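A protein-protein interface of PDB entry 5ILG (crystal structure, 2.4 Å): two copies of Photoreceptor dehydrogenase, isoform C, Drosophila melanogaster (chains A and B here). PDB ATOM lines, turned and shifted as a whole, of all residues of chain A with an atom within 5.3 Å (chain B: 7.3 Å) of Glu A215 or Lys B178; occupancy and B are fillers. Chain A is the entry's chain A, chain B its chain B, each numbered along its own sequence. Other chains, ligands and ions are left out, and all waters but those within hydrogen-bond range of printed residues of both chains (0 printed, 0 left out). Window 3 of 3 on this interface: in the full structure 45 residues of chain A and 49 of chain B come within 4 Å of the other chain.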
ATOM      1  N   PHE A 155      -1.008   6.320 -22.918  1.00  0.00           N
ATOM      2  CA  PHE A 155       0.015   5.907 -21.935  1.00  0.00           C
ATOM      3  C   PHE A 155       1.456   5.728 -22.463  1.00  0.00           C
ATOM      4  O   PHE A 155       2.385   5.863 -21.706  1.00  0.00           O
ATOM      5  CB  PHE A 155      -0.418   4.597 -21.251  1.00  0.00           C
ATOM      6  CG  PHE A 155      -0.293   3.373 -22.121  1.00  0.00           C
ATOM      7  CD1 PHE A 155      -1.310   3.048 -23.021  1.00  0.00           C
ATOM      8  CD2 PHE A 155       0.828   2.518 -22.023  1.00  0.00           C
ATOM      9  CE1 PHE A 155      -1.218   1.914 -23.812  1.00  0.00           C
ATOM     10  CE2 PHE A 155       0.926   1.373 -22.823  1.00  0.00           C
ATOM     11  CZ  PHE A 155      -0.107   1.069 -23.716  1.00  0.00           C
ATOM     12  N   ILE A 156       1.612   5.406 -23.741  1.00  0.00           N
ATOM     13  CA  ILE A 156       2.953   5.261 -24.357  1.00  0.00           C
ATOM     14  C   ILE A 156       3.720   6.578 -24.411  1.00  0.00           C
ATOM     15  O   ILE A 156       4.951   6.582 -24.374  1.00  0.00           O
ATOM     16  CB  ILE A 156       2.904   4.691 -25.790  1.00  0.00           C
ATOM     17  CG1 ILE A 156       2.246   3.334 -25.795  1.00  0.00           C
ATOM     18  CG2 ILE A 156       4.294   4.600 -26.414  1.00  0.00           C
ATOM     19  CD1 ILE A 156       1.996   2.787 -27.184  1.00  0.00           C
ATOM     20  N   THR A 212       7.508  -0.801 -23.873  1.00  0.00           N
ATOM     21  CA  THR A 212       6.213  -0.486 -24.525  1.00  0.00           C
ATOM     22  C   THR A 212       6.347  -0.419 -26.047  1.00  0.00           C
ATOM     23  O   THR A 212       5.405  -0.062 -26.738  1.00  0.00           O
ATOM     24  CB  THR A 212       5.578   0.834 -24.016  1.00  0.00           C
ATOM     25  OG1 THR A 212       6.402   1.938 -24.388  1.00  0.00           O
ATOM     26  CG2 THR A 212       5.431   0.824 -22.503  1.00  0.00           C
ATOM     27  N   SER A 213       7.512  -0.759 -26.577  1.00  0.00           N
ATOM     28  CA  SER A 213       7.712  -0.795 -28.048  1.00  0.00           C
ATOM     29  C   SER A 213       6.732  -1.754 -28.760  1.00  0.00           C
ATOM     30  O   SER A 213       6.223  -1.471 -29.844  1.00  0.00           O
ATOM     31  CB  SER A 213       9.149  -1.168 -28.378  1.00  0.00           C
ATOM     32  OG  SER A 213       9.357  -2.506 -28.051  1.00  0.00           O
ATOM     33  N   ASP A 214       6.418  -2.856 -28.097  1.00  0.00           N
ATOM     34  CA  ASP A 214       5.366  -3.798 -28.560  1.00  0.00           C
ATOM     35  C   ASP A 214       3.918  -3.271 -28.503  1.00  0.00           C
ATOM     36  O   ASP A 214       3.000  -3.961 -28.922  1.00  0.00           O
ATOM     37  CB  ASP A 214       5.464  -5.115 -27.768  1.00  0.00           C
ATOM     38  CG  ASP A 214       5.204  -4.936 -26.254  1.00  0.00           C
ATOM     39  OD1 ASP A 214       5.443  -3.839 -25.710  1.00  0.00           O
ATOM     40  OD2 ASP A 214       4.750  -5.894 -25.600  1.00  0.00           O
ATOM     41  N   GLU A 215       3.720  -2.072 -27.950  1.00  0.00           N
ATOM     42  CA  GLU A 215       2.397  -1.387 -27.899  1.00  0.00           C
ATOM     43  C   GLU A 215       2.254  -0.222 -28.907  1.00  0.00           C
ATOM     44  O   GLU A 215       1.152   0.299 -29.115  1.00  0.00           O
ATOM     45  CB  GLU A 215       2.117  -0.839 -26.496  1.00  0.00           C
ATOM     46  CG  GLU A 215       2.138  -1.893 -25.399  1.00  0.00           C
ATOM     47  CD  GLU A 215       1.016  -2.912 -25.518  1.00  0.00           C
ATOM     48  OE1 GLU A 215      -0.019  -2.615 -26.162  1.00  0.00           O
ATOM     49  OE2 GLU A 215       1.164  -3.999 -24.932  1.00  0.00           O
ATOM     50  N   THR A 216       3.364   0.162 -29.548  1.00  0.00           N
ATOM     51  CA  THR A 216       3.351   1.324 -30.475  1.00  0.00           C
ATOM     52  C   THR A 216       2.428   1.150 -31.685  1.00  0.00           C
ATOM     53  O   THR A 216       1.946   2.122 -32.249  1.00  0.00           O
ATOM     54  CB  THR A 216       4.742   1.691 -30.952  1.00  0.00           C
ATOM     55  OG1 THR A 216       5.305   0.573 -31.639  1.00  0.00           O
ATOM     56  CG2 THR A 216       5.612   2.072 -29.760  1.00  0.00           C
ATOM     57  N   TYR A 217       2.167  -0.102 -32.049  1.00  0.00           N
ATOM     58  CA  TYR A 217       1.222  -0.438 -33.118  1.00  0.00           C
ATOM     59  C   TYR A 217      -0.125   0.267 -32.924  1.00  0.00           C
ATOM     60  O   TYR A 217      -0.809   0.623 -33.888  1.00  0.00           O
ATOM     61  CB  TYR A 217       1.023  -1.971 -33.221  1.00  0.00           C
ATOM     62  CG  TYR A 217       0.121  -2.581 -32.150  1.00  0.00           C
ATOM     63  CD1 TYR A 217      -1.256  -2.701 -32.357  1.00  0.00           C
ATOM     64  CD2 TYR A 217       0.643  -3.031 -30.927  1.00  0.00           C
ATOM     65  CE1 TYR A 217      -2.090  -3.234 -31.383  1.00  0.00           C
ATOM     66  CE2 TYR A 217      -0.179  -3.575 -29.939  1.00  0.00           C
ATOM     67  CZ  TYR A 217      -1.546  -3.674 -30.171  1.00  0.00           C
ATOM     68  OH  TYR A 217      -2.387  -4.219 -29.223  1.00  0.00           O
ATOM     69  N   ARG A 218      -0.512   0.441 -31.671  1.00  0.00           N
ATOM     70  CA  ARG A 218      -1.773   1.123 -31.318  1.00  0.00           C
ATOM     71  C   ARG A 218      -1.906   2.497 -31.978  1.00  0.00           C
ATOM     72  O   ARG A 218      -2.993   2.925 -32.362  1.00  0.00           O
ATOM     73  CB  ARG A 218      -1.893   1.265 -29.804  1.00  0.00           C
ATOM     74  CG  ARG A 218      -2.257  -0.030 -29.078  1.00  0.00           C
ATOM     75  CD  ARG A 218      -2.006   0.097 -27.576  1.00  0.00           C
ATOM     76  NE  ARG A 218      -2.322  -1.108 -26.828  1.00  0.00           N
ATOM     77  CZ  ARG A 218      -3.542  -1.426 -26.397  1.00  0.00           C
ATOM     78  NH1 ARG A 218      -3.732  -2.550 -25.730  1.00  0.00           N
ATOM     79  NH2 ARG A 218      -4.586  -0.634 -26.635  1.00  0.00           N
ATOM     80  N   ILE A 219      -0.781   3.180 -32.091  1.00  0.00           N
ATOM     81  CA  ILE A 219      -0.707   4.457 -32.811  1.00  0.00           C
ATOM     82  C   ILE A 219      -0.404   4.246 -34.290  1.00  0.00           C
ATOM     83  O   ILE A 219      -1.130   4.751 -35.167  1.00  0.00           O
ATOM     84  CB  ILE A 219       0.362   5.360 -32.197  1.00  0.00           C
ATOM     85  CG1 ILE A 219      -0.011   5.642 -30.742  1.00  0.00           C
ATOM     86  CG2 ILE A 219       0.503   6.656 -32.990  1.00  0.00           C
ATOM     87  CD1 ILE A 219       1.042   6.431 -30.009  1.00  0.00           C
ATOM     88  N   LEU B 174       0.988   7.142 -16.720  1.00  0.00           N
ATOM     89  CA  LEU B 174       1.872   6.209 -16.006  1.00  0.00           C
ATOM     90  C   LEU B 174       1.121   5.169 -15.190  1.00  0.00           C
ATOM     91  O   LEU B 174       1.673   4.132 -14.822  1.00  0.00           O
ATOM     92  CB  LEU B 174       2.853   6.977 -15.111  1.00  0.00           C
ATOM     93  CG  LEU B 174       3.838   7.924 -15.824  1.00  0.00           C
ATOM     94  CD1 LEU B 174       4.911   8.429 -14.865  1.00  0.00           C
ATOM     95  CD2 LEU B 174       4.533   7.280 -16.986  1.00  0.00           C
ATOM     96  N   ALA B 175      -0.155   5.451 -14.943  1.00  0.00           N
ATOM     97  CA  ALA B 175      -1.025   4.558 -14.184  1.00  0.00           C
ATOM     98  C   ALA B 175      -1.621   3.444 -15.015  1.00  0.00           C
ATOM     99  O   ALA B 175      -2.422   2.671 -14.520  1.00  0.00           O
ATOM    100  CB  ALA B 175      -2.142   5.353 -13.540  1.00  0.00           C
ATOM    101  N   ASN B 176      -1.253   3.352 -16.273  1.00  0.00           N
ATOM    102  CA  ASN B 176      -1.764   2.296 -17.121  1.00  0.00           C
ATOM    103  C   ASN B 176      -1.385   0.893 -16.600  1.00  0.00           C
ATOM    104  O   ASN B 176      -0.278   0.678 -16.117  1.00  0.00           O
ATOM    105  CB  ASN B 176      -1.266   2.474 -18.557  1.00  0.00           C
ATOM    106  CG  ASN B 176      -2.116   1.703 -19.556  1.00  0.00           C
ATOM    107  OD1 ASN B 176      -1.829   0.541 -19.858  1.00  0.00           O
ATOM    108  ND2 ASN B 176      -3.167   2.339 -20.070  1.00  0.00           N
ATOM    109  N   GLU B 177      -2.313  -0.045 -16.746  1.00  0.00           N
ATOM    110  CA  GLU B 177      -2.131  -1.451 -16.297  1.00  0.00           C
ATOM    111  C   GLU B 177      -0.824  -2.100 -16.804  1.00  0.00           C
ATOM    112  O   GLU B 177      -0.172  -2.867 -16.098  1.00  0.00           O
ATOM    113  CB  GLU B 177      -3.313  -2.313 -16.766  1.00  0.00           C
ATOM    114  CG  GLU B 177      -3.648  -3.466 -15.843  1.00  0.00           C
ATOM    115  CD  GLU B 177      -4.238  -3.004 -14.512  1.00  0.00           C
ATOM    116  OE1 GLU B 177      -3.954  -3.637 -13.468  1.00  0.00           O
ATOM    117  OE2 GLU B 177      -4.966  -1.988 -14.501  1.00  0.00           O
ATOM    118  N   LYS B 178      -0.458  -1.754 -18.034  1.00  0.00           N
ATOM    119  CA  LYS B 178       0.802  -2.199 -18.660  1.00  0.00           C
ATOM    120  C   LYS B 178       2.000  -1.970 -17.767  1.00  0.00           C
ATOM    121  O   LYS B 178       2.769  -2.884 -17.563  1.00  0.00           O
ATOM    122  CB  LYS B 178       1.073  -1.464 -19.979  1.00  0.00           C
ATOM    123  CG  LYS B 178       0.049  -1.721 -21.069  1.00  0.00           C
ATOM    124  CD  LYS B 178       0.010  -3.168 -21.542  1.00  0.00           C
ATOM    125  CE  LYS B 178      -0.980  -3.338 -22.694  1.00  0.00           C
ATOM    126  NZ  LYS B 178      -2.386  -2.958 -22.381  1.00  0.00           N
ATOM    127  N   TYR B 179       2.116  -0.742 -17.248  1.00  0.00           N
ATOM    128  CA  TYR B 179       3.196  -0.350 -16.338  1.00  0.00           C
ATOM    129  C   TYR B 179       3.021  -0.978 -14.972  1.00  0.00           C
ATOM    130  O   TYR B 179       3.970  -1.423 -14.387  1.00  0.00           O
ATOM    131  CB  TYR B 179       3.274   1.168 -16.164  1.00  0.00           C
ATOM    132  CG  TYR B 179       3.487   1.957 -17.437  1.00  0.00           C
ATOM    133  CD1 TYR B 179       4.635   1.776 -18.214  1.00  0.00           C
ATOM    134  CD2 TYR B 179       2.548   2.899 -17.865  1.00  0.00           C
ATOM    135  CE1 TYR B 179       4.841   2.505 -19.382  1.00  0.00           C
ATOM    136  CE2 TYR B 179       2.749   3.641 -19.017  1.00  0.00           C
ATOM    137  CZ  TYR B 179       3.895   3.447 -19.788  1.00  0.00           C
ATOM    138  OH  TYR B 179       4.105   4.195 -20.956  1.00  0.00           O
ATOM    139  N   TYR B 180       1.794  -1.013 -14.474  1.00  0.00           N
ATOM    140  CA  TYR B 180       1.549  -1.417 -13.085  1.00  0.00           C
ATOM    141  C   TYR B 180       1.947  -2.864 -12.794  1.00  0.00           C
ATOM    142  O   TYR B 180       2.627  -3.138 -11.800  1.00  0.00           O
ATOM    143  CB  TYR B 180       0.084  -1.217 -12.688  1.00  0.00           C
ATOM    144  CG  TYR B 180      -0.172  -1.626 -11.264  1.00  0.00           C
ATOM    145  CD1 TYR B 180       0.450  -0.965 -10.210  1.00  0.00           C
ATOM    146  CD2 TYR B 180      -0.986  -2.704 -10.973  1.00  0.00           C
ATOM    147  CE1 TYR B 180       0.251  -1.367  -8.904  1.00  0.00           C
ATOM    148  CE2 TYR B 180      -1.188  -3.119  -9.675  1.00  0.00           C
ATOM    149  CZ  TYR B 180      -0.571  -2.440  -8.651  1.00  0.00           C
ATOM    150  OH  TYR B 180      -0.763  -2.837  -7.361  1.00  0.00           O
ATOM    151  N   GLN B 181       1.530  -3.760 -13.679  1.00  0.00           N
ATOM    152  CA  GLN B 181       1.861  -5.184 -13.570  1.00  0.00           C
ATOM    153  C   GLN B 181       3.357  -5.440 -13.464  1.00  0.00           C
ATOM    154  O   GLN B 181       3.792  -6.317 -12.729  1.00  0.00           O
ATOM    155  CB  GLN B 181       1.318  -5.958 -14.770  1.00  0.00           C
ATOM    156  CG  GLN B 181      -0.203  -5.918 -14.929  1.00  0.00           C
ATOM    157  CD  GLN B 181      -0.967  -6.092 -13.617  1.00  0.00           C
ATOM    158  OE1 GLN B 181      -1.868  -5.310 -13.320  1.00  0.00           O
ATOM    159  NE2 GLN B 181      -0.605  -7.110 -12.834  1.00  0.00           N
ATOM    160  N   ARG B 182       4.129  -4.658 -14.199  1.00  0.00           N
ATOM    161  CA  ARG B 182       5.577  -4.792 -14.249  1.00  0.00           C
ATOM    162  C   ARG B 182       6.271  -4.131 -13.055  1.00  0.00           C
ATOM    163  O   ARG B 182       7.176  -4.706 -12.466  1.00  0.00           O
ATOM    164  CB  ARG B 182       6.085  -4.201 -15.578  1.00  0.00           C
ATOM    165  CG  ARG B 182       7.591  -3.962 -15.729  1.00  0.00           C
ATOM    166  CD  ARG B 182       7.988  -3.228 -17.030  1.00  0.00           C
ATOM    167  NE  ARG B 182       6.898  -2.458 -17.665  1.00  0.00           N
ATOM    168  CZ  ARG B 182       6.097  -2.908 -18.646  1.00  0.00           C
ATOM    169  NH1 ARG B 182       6.264  -4.133 -19.176  1.00  0.00           N
ATOM    170  NH2 ARG B 182       5.144  -2.112 -19.140  1.00  0.00           N
ATOM    171  N   SER B 183       5.863  -2.914 -12.724  1.00  0.00           N
ATOM    172  CA  SER B 183       6.557  -2.103 -11.710  1.00  0.00           C
ATOM    173  C   SER B 183       5.941  -2.211 -10.313  1.00  0.00           C
ATOM    174  O   SER B 183       6.627  -2.079  -9.302  1.00  0.00           O
ATOM    175  CB  SER B 183       6.624  -0.624 -12.136  1.00  0.00           C
ATOM    176  OG  SER B 183       5.357   0.010 -12.115  1.00  0.00           O
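The side-chain hydroxyl (OH) of Tyr B179 is in hydrogen-bond range of the backbone carbonyl oxygen (O) of Phe A155 (2.5 Å).
The side-chain carboxylate (OE1) of Glu A215 lies within salt-bridge range of the guanidinium group (NE) of Arg A218, 2.8 Å away. The side-chain amide oxygen of Asn B176 sits close to the backbone NH of Lys B178, 3.2 Å away. O of Lys B178 lies within hydrogen-bond range of NH2 of Arg B182, 3.0 Å away. O of Tyr B179 lies within hydrogen-bond range of OG of Ser B183, at 3.0 Å.
Phe A155 touches Asn B176 (CB to CB, 3.5 Å). Lys B178 touches Phe A155. Ile A156 touches Tyr B179 (CA to OH, 3.7 Å). Tyr B179 touches Thr A212. Glu A215 touches Lys B178 (OE2 to CE, 3.2 Å). Lys B178 touches Arg A218.
Of chain B, only Lys B178 (3.2 Å) comes within 4 Å of Glu A215. Of chain A, only Phe A155, Glu A215 and Arg A218 come within 4 Å of Lys B178. Of the printed residues of chain B, Thr A212 touches Tyr B179. Printed residues of chain B within 4 Å of Phe A155: Asn B176, Lys B178 and Tyr B179. Printed residues of chain A within 4 Å of Asn B176: Phe A155. Of the printed residues of chain A, Tyr B179 touches Phe A155 (2.5 Å), Ile A156 (3.7 Å) and Thr A212 (3.6 Å). The nearest residue of chain B that does not touch Glu A215 is Arg B182 (6.9 Å).
Of the 10 printed residues of chain B, 3 touch a printed residue of chain A. Along chain B the printed residues that touch a printed residue of chain A span positions 176 to 179. Hydrophobic or aromatic side chains of chain A within 4 Å of the printed part of chain B: Phe A155. Among the printed residues, no Asp or Glu carboxylate lies within 4 Å of a Lys or Arg side-chain nitrogen of the other chain.
No position is printed for both chains. Of the 7 pairs that touch across the chains among the printed residues, none has its exchanged pair printed and touching as well.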
